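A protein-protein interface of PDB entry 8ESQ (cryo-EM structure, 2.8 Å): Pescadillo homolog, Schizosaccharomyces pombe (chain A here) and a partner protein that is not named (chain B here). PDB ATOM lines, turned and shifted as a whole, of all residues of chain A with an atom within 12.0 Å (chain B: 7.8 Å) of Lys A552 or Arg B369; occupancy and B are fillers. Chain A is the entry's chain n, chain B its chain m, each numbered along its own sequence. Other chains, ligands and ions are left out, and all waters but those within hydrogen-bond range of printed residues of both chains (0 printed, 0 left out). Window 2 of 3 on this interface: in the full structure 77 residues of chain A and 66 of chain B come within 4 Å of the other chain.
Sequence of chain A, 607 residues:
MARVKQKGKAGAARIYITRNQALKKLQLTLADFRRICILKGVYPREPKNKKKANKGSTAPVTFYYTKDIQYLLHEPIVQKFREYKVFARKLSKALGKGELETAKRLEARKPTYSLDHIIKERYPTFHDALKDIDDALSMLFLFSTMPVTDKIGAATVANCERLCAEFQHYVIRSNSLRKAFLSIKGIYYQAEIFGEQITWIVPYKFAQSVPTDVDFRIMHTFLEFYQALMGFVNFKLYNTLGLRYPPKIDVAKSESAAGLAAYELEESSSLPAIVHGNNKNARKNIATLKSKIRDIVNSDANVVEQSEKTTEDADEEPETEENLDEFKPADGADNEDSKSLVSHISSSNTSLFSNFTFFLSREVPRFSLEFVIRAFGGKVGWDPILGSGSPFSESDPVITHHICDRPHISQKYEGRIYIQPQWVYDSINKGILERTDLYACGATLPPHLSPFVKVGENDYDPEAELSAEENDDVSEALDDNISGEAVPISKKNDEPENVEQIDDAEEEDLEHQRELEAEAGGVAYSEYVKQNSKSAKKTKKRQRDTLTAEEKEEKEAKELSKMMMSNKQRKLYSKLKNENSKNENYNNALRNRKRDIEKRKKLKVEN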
ATOM      1  N   ALA A 549      14.710  24.296 -27.321  1.00  0.00           N
ATOM      2  CA  ALA A 549      13.379  24.890 -27.363  1.00  0.00           C
ATOM      3  C   ALA A 549      12.511  24.207 -28.413  1.00  0.00           C
ATOM      4  O   ALA A 549      11.490  23.600 -28.089  1.00  0.00           O
ATOM      5  CB  ALA A 549      13.472  26.382 -27.639  1.00  0.00           C
ATOM      6  N   GLU A 550      12.924  24.318 -29.677  1.00  0.00           N
ATOM      7  CA  GLU A 550      12.176  23.679 -30.754  1.00  0.00           C
ATOM      8  C   GLU A 550      12.236  22.160 -30.641  1.00  0.00           C
ATOM      9  O   GLU A 550      11.261  21.468 -30.957  1.00  0.00           O
ATOM     10  CB  GLU A 550      12.704  24.147 -32.114  1.00  0.00           C
ATOM     11  CG  GLU A 550      14.103  23.657 -32.472  1.00  0.00           C
ATOM     12  CD  GLU A 550      15.206  24.520 -31.886  1.00  0.00           C
ATOM     13  OE1 GLU A 550      14.930  25.293 -30.946  1.00  0.00           O
ATOM     14  OE2 GLU A 550      16.354  24.422 -32.369  1.00  0.00           O
ATOM     15  N   GLU A 551      13.375  21.624 -30.195  1.00  0.00           N
ATOM     16  CA  GLU A 551      13.507  20.178 -30.058  1.00  0.00           C
ATOM     17  C   GLU A 551      12.566  19.631 -28.993  1.00  0.00           C
ATOM     18  O   GLU A 551      11.917  18.601 -29.202  1.00  0.00           O
ATOM     19  CB  GLU A 551      14.955  19.809 -29.738  1.00  0.00           C
ATOM     20  CG  GLU A 551      15.936  20.129 -30.853  1.00  0.00           C
ATOM     21  CD  GLU A 551      15.612  19.400 -32.142  1.00  0.00           C
ATOM     22  OE1 GLU A 551      15.121  18.253 -32.074  1.00  0.00           O
ATOM     23  OE2 GLU A 551      15.846  19.975 -33.227  1.00  0.00           O
ATOM     24  N   LYS A 552      12.467  20.316 -27.850  1.00  0.00           N
ATOM     25  CA  LYS A 552      11.632  19.828 -26.757  1.00  0.00           C
ATOM     26  C   LYS A 552      10.154  19.803 -27.122  1.00  0.00           C
ATOM     27  O   LYS A 552       9.378  19.101 -26.467  1.00  0.00           O
ATOM     28  CB  LYS A 552      11.849  20.683 -25.506  1.00  0.00           C
ATOM     29  CG  LYS A 552      10.856  21.824 -25.342  1.00  0.00           C
ATOM     30  CD  LYS A 552      10.864  22.362 -23.921  1.00  0.00           C
ATOM     31  CE  LYS A 552      12.161  23.090 -23.611  1.00  0.00           C
ATOM     32  NZ  LYS A 552      12.201  24.441 -24.233  1.00  0.00           N
ATOM     33  N   GLU A 553       9.749  20.548 -28.148  1.00  0.00           N
ATOM     34  CA  GLU A 553       8.381  20.509 -28.649  1.00  0.00           C
ATOM     35  C   GLU A 553       8.217  19.556 -29.824  1.00  0.00           C
ATOM     36  O   GLU A 553       7.204  18.855 -29.910  1.00  0.00           O
ATOM     37  CB  GLU A 553       7.930  21.914 -29.064  1.00  0.00           C
ATOM     38  CG  GLU A 553       6.531  21.972 -29.655  1.00  0.00           C
ATOM     39  CD  GLU A 553       5.449  21.809 -28.608  1.00  0.00           C
ATOM     40  OE1 GLU A 553       5.706  22.133 -27.430  1.00  0.00           O
ATOM     41  OE2 GLU A 553       4.340  21.359 -28.964  1.00  0.00           O
ATOM     42  N   GLU A 554       9.199  19.507 -30.726  1.00  0.00           N
ATOM     43  CA  GLU A 554       9.115  18.592 -31.860  1.00  0.00           C
ATOM     44  C   GLU A 554       9.183  17.139 -31.410  1.00  0.00           C
ATOM     45  O   GLU A 554       8.543  16.271 -32.014  1.00  0.00           O
ATOM     46  CB  GLU A 554      10.224  18.890 -32.868  1.00  0.00           C
ATOM     47  CG  GLU A 554      10.013  20.156 -33.678  1.00  0.00           C
ATOM     48  CD  GLU A 554      11.097  20.366 -34.717  1.00  0.00           C
ATOM     49  OE1 GLU A 554      12.038  19.547 -34.765  1.00  0.00           O
ATOM     50  OE2 GLU A 554      11.006  21.346 -35.485  1.00  0.00           O
ATOM     51  N   LYS A 555       9.967  16.849 -30.367  1.00  0.00           N
ATOM     52  CA  LYS A 555      10.077  15.469 -29.904  1.00  0.00           C
ATOM     53  C   LYS A 555       8.731  14.948 -29.418  1.00  0.00           C
ATOM     54  O   LYS A 555       8.316  13.846 -29.787  1.00  0.00           O
ATOM     55  CB  LYS A 555      11.154  15.347 -28.817  1.00  0.00           C
ATOM     56  CG  LYS A 555      10.966  16.207 -27.574  1.00  0.00           C
ATOM     57  CD  LYS A 555      10.334  15.434 -26.434  1.00  0.00           C
ATOM     58  CE  LYS A 555      10.269  16.276 -25.172  1.00  0.00           C
ATOM     59  NZ  LYS A 555       9.624  15.530 -24.060  1.00  0.00           N
ATOM     60  N   GLU A 556       8.011  15.741 -28.621  1.00  0.00           N
ATOM     61  CA  GLU A 556       6.674  15.324 -28.211  1.00  0.00           C
ATOM     62  C   GLU A 556       5.716  15.306 -29.392  1.00  0.00           C
ATOM     63  O   GLU A 556       4.832  14.445 -29.470  1.00  0.00           O
ATOM     64  CB  GLU A 556       6.144  16.226 -27.096  1.00  0.00           C
ATOM     65  CG  GLU A 556       6.847  16.020 -25.772  1.00  0.00           C
ATOM     66  CD  GLU A 556       6.821  14.566 -25.335  1.00  0.00           C
ATOM     67  OE1 GLU A 556       5.749  13.936 -25.435  1.00  0.00           O
ATOM     68  OE2 GLU A 556       7.875  14.047 -24.913  1.00  0.00           O
ATOM     69  N   ALA A 557       5.871  16.253 -30.320  1.00  0.00           N
ATOM     70  CA  ALA A 557       4.961  16.333 -31.459  1.00  0.00           C
ATOM     71  C   ALA A 557       5.029  15.087 -32.331  1.00  0.00           C
ATOM     72  O   ALA A 557       4.023  14.702 -32.939  1.00  0.00           O
ATOM     73  CB  ALA A 557       5.264  17.583 -32.284  1.00  0.00           C
ATOM     74  N   LYS A 558       6.194  14.446 -32.406  1.00  0.00           N
ATOM     75  CA  LYS A 558       6.382  13.240 -33.200  1.00  0.00           C
ATOM     76  C   LYS A 558       6.406  11.963 -32.366  1.00  0.00           C
ATOM     77  O   LYS A 558       6.457  10.873 -32.940  1.00  0.00           O
ATOM     78  CB  LYS A 558       7.657  13.395 -34.071  1.00  0.00           C
ATOM     79  CG  LYS A 558       9.071  13.055 -33.490  1.00  0.00           C
ATOM     80  CD  LYS A 558       9.343  11.611 -33.062  1.00  0.00           C
ATOM     81  CE  LYS A 558      10.683  11.455 -32.363  1.00  0.00           C
ATOM     82  NZ  LYS A 558      10.983  10.010 -32.118  1.00  0.00           N
ATOM     83  N   GLU A 559       6.308  12.053 -31.041  1.00  0.00           N
ATOM     84  CA  GLU A 559       6.444  10.867 -30.210  1.00  0.00           C
ATOM     85  C   GLU A 559       5.152  10.466 -29.516  1.00  0.00           C
ATOM     86  O   GLU A 559       5.054   9.334 -29.034  1.00  0.00           O
ATOM     87  CB  GLU A 559       7.559  11.071 -29.174  1.00  0.00           C
ATOM     88  CG  GLU A 559       7.940   9.839 -28.370  1.00  0.00           C
ATOM     89  CD  GLU A 559       7.469   9.928 -26.939  1.00  0.00           C
ATOM     90  OE1 GLU A 559       7.348  11.062 -26.432  1.00  0.00           O
ATOM     91  OE2 GLU A 559       7.208   8.872 -26.327  1.00  0.00           O
ATOM     92  N   LEU A 560       4.149  11.332 -29.529  1.00  0.00           N
ATOM     93  CA  LEU A 560       2.866  10.940 -28.966  1.00  0.00           C
ATOM     94  C   LEU A 560       2.102  10.077 -29.966  1.00  0.00           C
ATOM     95  O   LEU A 560       1.923   8.881 -29.733  1.00  0.00           O
ATOM     96  CB  LEU A 560       2.061  12.176 -28.514  1.00  0.00           C
ATOM     97  CG  LEU A 560       1.116  12.975 -29.420  1.00  0.00           C
ATOM     98  CD1 LEU A 560       0.137  13.797 -28.595  1.00  0.00           C
ATOM     99  CD2 LEU A 560       1.879  13.862 -30.392  1.00  0.00           C
ATOM    100  N   THR B 364       0.362  20.137 -26.749  1.00  0.00           N
ATOM    101  CA  THR B 364       0.746  21.337 -26.015  1.00  0.00           C
ATOM    102  C   THR B 364       1.584  20.984 -24.782  1.00  0.00           C
ATOM    103  O   THR B 364       1.194  21.292 -23.652  1.00  0.00           O
ATOM    104  CB  THR B 364      -0.477  22.154 -25.619  1.00  0.00           C
ATOM    105  OG1 THR B 364      -1.236  21.440 -24.635  1.00  0.00           O
ATOM    106  CG2 THR B 364      -1.352  22.428 -26.833  1.00  0.00           C
ATOM    107  N   PRO B 365       2.732  20.318 -24.964  1.00  0.00           N
ATOM    108  CA  PRO B 365       3.542  19.943 -23.792  1.00  0.00           C
ATOM    109  C   PRO B 365       4.126  21.136 -23.063  1.00  0.00           C
ATOM    110  O   PRO B 365       4.384  21.050 -21.856  1.00  0.00           O
ATOM    111  CB  PRO B 365       4.639  19.058 -24.396  1.00  0.00           C
ATOM    112  CG  PRO B 365       4.773  19.541 -25.788  1.00  0.00           C
ATOM    113  CD  PRO B 365       3.399  19.958 -26.227  1.00  0.00           C
ATOM    114  N   SER B 366       4.361  22.245 -23.767  1.00  0.00           N
ATOM    115  CA  SER B 366       4.877  23.441 -23.110  1.00  0.00           C
ATOM    116  C   SER B 366       3.859  24.017 -22.135  1.00  0.00           C
ATOM    117  O   SER B 366       4.226  24.526 -21.070  1.00  0.00           O
ATOM    118  CB  SER B 366       5.274  24.481 -24.156  1.00  0.00           C
ATOM    119  OG  SER B 366       4.174  24.817 -24.982  1.00  0.00           O
ATOM    120  N   GLU B 367       2.573  23.957 -22.486  1.00  0.00           N
ATOM    121  CA  GLU B 367       1.540  24.478 -21.597  1.00  0.00           C
ATOM    122  C   GLU B 367       1.463  23.671 -20.307  1.00  0.00           C
ATOM    123  O   GLU B 367       1.176  24.220 -19.237  1.00  0.00           O
ATOM    124  CB  GLU B 367       0.188  24.486 -22.314  1.00  0.00           C
ATOM    125  CG  GLU B 367       0.005  25.623 -23.318  1.00  0.00           C
ATOM    126  CD  GLU B 367       1.048  25.625 -24.425  1.00  0.00           C
ATOM    127  OE1 GLU B 367       1.525  24.535 -24.804  1.00  0.00           O
ATOM    128  OE2 GLU B 367       1.395  26.722 -24.913  1.00  0.00           O
ATOM    129  N   LEU B 368       1.714  22.368 -20.390  1.00  0.00           N
ATOM    130  CA  LEU B 368       1.687  21.464 -19.243  1.00  0.00           C
ATOM    131  C   LEU B 368       3.090  20.892 -19.043  1.00  0.00           C
ATOM    132  O   LEU B 368       3.452  19.851 -19.586  1.00  0.00           O
ATOM    133  CB  LEU B 368       0.577  20.373 -19.460  1.00  0.00           C
ATOM    134  CG  LEU B 368       0.439  19.508 -20.730  1.00  0.00           C
ATOM    135  CD1 LEU B 368       1.332  18.270 -20.800  1.00  0.00           C
ATOM    136  CD2 LEU B 368      -1.023  19.127 -20.935  1.00  0.00           C
ATOM    137  N   ARG B 369       3.894  21.591 -18.236  1.00  0.00           N
ATOM    138  CA  ARG B 369       5.321  21.295 -18.108  1.00  0.00           C
ATOM    139  C   ARG B 369       5.739  21.080 -16.655  1.00  0.00           C
ATOM    140  O   ARG B 369       6.513  21.875 -16.101  1.00  0.00           O
ATOM    141  CB  ARG B 369       6.157  22.414 -18.729  1.00  0.00           C
ATOM    142  CG  ARG B 369       5.731  23.817 -18.314  1.00  0.00           C
ATOM    143  CD  ARG B 369       6.527  24.896 -19.034  1.00  0.00           C
ATOM    144  NE  ARG B 369       6.748  24.585 -20.442  1.00  0.00           N
ATOM    145  CZ  ARG B 369       7.936  24.325 -20.970  1.00  0.00           C
ATOM    146  NH1 ARG B 369       9.037  24.353 -20.238  1.00  0.00           N
ATOM    147  NH2 ARG B 369       8.023  24.038 -22.266  1.00  0.00           N
ATOM    148  N   PRO B 370       5.260  20.013 -16.001  1.00  0.00           N
ATOM    149  CA  PRO B 370       5.988  19.515 -14.829  1.00  0.00           C
ATOM    150  C   PRO B 370       6.983  18.443 -15.242  1.00  0.00           C
ATOM    151  O   PRO B 370       7.090  17.401 -14.590  1.00  0.00           O
ATOM    152  CB  PRO B 370       4.878  18.950 -13.933  1.00  0.00           C
ATOM    153  CG  PRO B 370       3.680  18.748 -14.840  1.00  0.00           C
ATOM    154  CD  PRO B 370       4.008  19.270 -16.213  1.00  0.00           C
ATOM    155  N   PHE B 371       7.727  18.692 -16.312  1.00  0.00           N
ATOM    156  CA  PHE B 371       8.524  17.634 -16.925  1.00  0.00           C
ATOM    157  C   PHE B 371       9.785  17.379 -16.113  1.00  0.00           C
ATOM    158  O   PHE B 371      10.455  18.338 -15.706  1.00  0.00           O
ATOM    159  CB  PHE B 371       8.876  17.989 -18.373  1.00  0.00           C
ATOM    160  CG  PHE B 371       9.647  19.271 -18.523  1.00  0.00           C
ATOM    161  CD1 PHE B 371      11.032  19.281 -18.437  1.00  0.00           C
ATOM    162  CD2 PHE B 371       8.994  20.455 -18.800  1.00  0.00           C
ATOM    163  CE1 PHE B 371      11.741  20.455 -18.583  1.00  0.00           C
ATOM    164  CE2 PHE B 371       9.699  21.631 -18.946  1.00  0.00           C
ATOM    165  CZ  PHE B 371      11.074  21.632 -18.841  1.00  0.00           C
ATOM    166  N   PRO B 372      10.127  16.130 -15.824  1.00  0.00           N
ATOM    167  CA  PRO B 372      11.431  15.850 -15.215  1.00  0.00           C
ATOM    168  C   PRO B 372      12.558  15.938 -16.232  1.00  0.00           C
ATOM    169  O   PRO B 372      12.705  15.060 -17.087  1.00  0.00           O
ATOM    170  CB  PRO B 372      11.269  14.427 -14.667  1.00  0.00           C
ATOM    171  CG  PRO B 372      10.183  13.826 -15.479  1.00  0.00           C
ATOM    172  CD  PRO B 372       9.269  14.937 -15.896  1.00  0.00           C
ATOM    173  N   THR B 373      13.363  16.997 -16.143  1.00  0.00           N
ATOM    174  CA  THR B 373      14.480  17.196 -17.059  1.00  0.00           C
ATOM    175  C   THR B 373      15.614  16.220 -16.762  1.00  0.00           C
ATOM    176  O   THR B 373      15.463  15.323 -15.926  1.00  0.00           O
ATOM    177  CB  THR B 373      14.973  18.647 -16.993  1.00  0.00           C
ATOM    178  OG1 THR B 373      15.707  18.963 -18.182  1.00  0.00           O
ATOM    179  CG2 THR B 373      15.854  18.883 -15.767  1.00  0.00           C
ATOM    180  N   LEU B 669       1.008  14.813  -8.375  1.00  0.00           N
ATOM    181  CA  LEU B 669       1.086  15.384  -9.709  1.00  0.00           C
ATOM    182  C   LEU B 669       0.495  14.416 -10.732  1.00  0.00           C
ATOM    183  O   LEU B 669       0.598  13.195 -10.564  1.00  0.00           O
ATOM    184  CB  LEU B 669       2.537  15.709 -10.066  1.00  0.00           C
ATOM    185  CG  LEU B 669       3.045  17.068  -9.588  1.00  0.00           C
ATOM    186  CD1 LEU B 669       4.547  17.172  -9.776  1.00  0.00           C
ATOM    187  CD2 LEU B 669       2.333  18.193 -10.320  1.00  0.00           C
ATOM    188  N   LEU B 671       1.308  12.855 -13.294  1.00  0.00           N
ATOM    189  CA  LEU B 671       2.360  12.283 -14.118  1.00  0.00           C
ATOM    190  C   LEU B 671       2.619  10.847 -13.690  1.00  0.00           C
ATOM    191  O   LEU B 671       2.556  10.512 -12.505  1.00  0.00           O
ATOM    192  CB  LEU B 671       3.660  13.090 -14.013  1.00  0.00           C
ATOM    193  CG  LEU B 671       3.556  14.599 -14.221  1.00  0.00           C
ATOM    194  CD1 LEU B 671       4.899  15.245 -13.957  1.00  0.00           C
ATOM    195  CD2 LEU B 671       3.069  14.923 -15.620  1.00  0.00           C
ATOM    196  N   HIS B 685       2.188  12.475 -19.147  1.00  0.00           N
ATOM    197  CA  HIS B 685       1.270  13.353 -18.433  1.00  0.00           C
ATOM    198  C   HIS B 685      -0.119  12.727 -18.456  1.00  0.00           C
ATOM    199  O   HIS B 685      -0.801  12.752 -19.485  1.00  0.00           O
ATOM    200  CB  HIS B 685       1.244  14.743 -19.060  1.00  0.00           C
ATOM    201  CG  HIS B 685       0.106  15.590 -18.585  1.00  0.00           C
ATOM    202  ND1 HIS B 685      -0.120  15.850 -17.251  1.00  0.00           N
ATOM    203  CD2 HIS B 685      -0.890  16.206 -19.263  1.00  0.00           C
ATOM    204  CE1 HIS B 685      -1.192  16.611 -17.129  1.00  0.00           C
ATOM    205  NE2 HIS B 685      -1.679  16.841 -18.335  1.00  0.00           N
ATOM    206  N   LEU B 701       5.369  12.949 -22.152  1.00  0.00           N
ATOM    207  CA  LEU B 701       5.993  14.194 -21.727  1.00  0.00           C
ATOM    208  C   LEU B 701       7.500  14.170 -21.953  1.00  0.00           C
ATOM    209  O   LEU B 701       8.090  15.193 -22.312  1.00  0.00           O
ATOM    210  CB  LEU B 701       5.667  14.468 -20.258  1.00  0.00           C
ATOM    211  CG  LEU B 701       5.936  15.889 -19.770  1.00  0.00           C
ATOM    212  CD1 LEU B 701       5.103  16.878 -20.564  1.00  0.00           C
ATOM    213  CD2 LEU B 701       5.613  15.996 -18.292  1.00  0.00           C
ATOM    214  N   LYS B 702       8.130  13.013 -21.757  1.00  0.00           N
ATOM    215  CA  LYS B 702       9.572  12.902 -21.924  1.00  0.00           C
ATOM    216  C   LYS B 702       9.956  11.433 -22.018  1.00  0.00           C
ATOM    217  O   LYS B 702       9.233  10.551 -21.547  1.00  0.00           O
ATOM    218  CB  LYS B 702      10.319  13.585 -20.770  1.00  0.00           C
ATOM    219  CG  LYS B 702      11.805  13.817 -21.012  1.00  0.00           C
ATOM    220  CD  LYS B 702      12.062  14.565 -22.305  1.00  0.00           C
ATOM    221  CE  LYS B 702      13.461  14.291 -22.830  1.00  0.00           C
ATOM    222  NZ  LYS B 702      13.633  12.868 -23.230  1.00  0.00           N
ATOM    223  N   ALA B 725       7.841  16.901  -9.113  1.00  0.00           N
ATOM    224  CA  ALA B 725       8.094  16.011 -10.244  1.00  0.00           C
ATOM    225  C   ALA B 725       9.562  15.589 -10.245  1.00  0.00           C
ATOM    226  O   ALA B 725      10.378  16.016 -11.066  1.00  0.00           O
ATOM    227  CB  ALA B 725       7.706  16.686 -11.552  1.00  0.00           C
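The side-chain carboxylate of Glu A556 sits at hydrogen-bond distance from the backbone NH of Lys B702 (3.3 Å). NZ of Lys A555 lies close to O of Leu B701, at 2.3 Å. N of Leu B701 sits at hydrogen-bond distance from OE1 of Glu A556, at 3.4 Å.
OG of Ser B366 sits at hydrogen-bond distance from OE1 of Glu B367 (2.7 Å). NZ of Lys A555 lies within salt-bridge range of OE2 of Glu A556 (2.4 Å). NE of Arg B369 is in hydrogen-bond range of O of Ser B366, at 2.6 Å.
Among the printed residues, merely in contact across the chains: Lys A552 with Arg B369 (3.7 Å), Glu A553 with Pro B365 (3.2 Å), Glu A553 with Ser B366 (3.9 Å), Lys A555 with Lys B702 (3.2 Å) and Glu A556 with Pro B365 (3.8 Å).
Lys A552 touches just one residue of chain B: Arg B369 (3.7 Å). Of the printed residues of chain A, Arg B369 touches Lys A552 (3.7 Å). Ser B366 touches just one residue of chain A: Glu A553 (3.9 Å). No residue of chain A comes within 4 Å of Leu B368. No residue of chain A comes within 4 Å of Pro B370. No residue of chain A comes within 4 Å of Phe B371. Of the printed residues of chain B, Glu A553 touches Pro B365 and Ser B366. Of the printed residues of chain B, Glu A556 touches Pro B365, Leu B701 and Lys B702. Printed residues of chain A within 4 Å of Leu B701: Lys A555 and Glu A556. Thr B364 touches none of the printed residues of chain A. Lys A558 touches none of the printed residues of chain B.
Hydrophobic or aromatic side chains of chain B that line the printed part of chain A: Pro B365.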
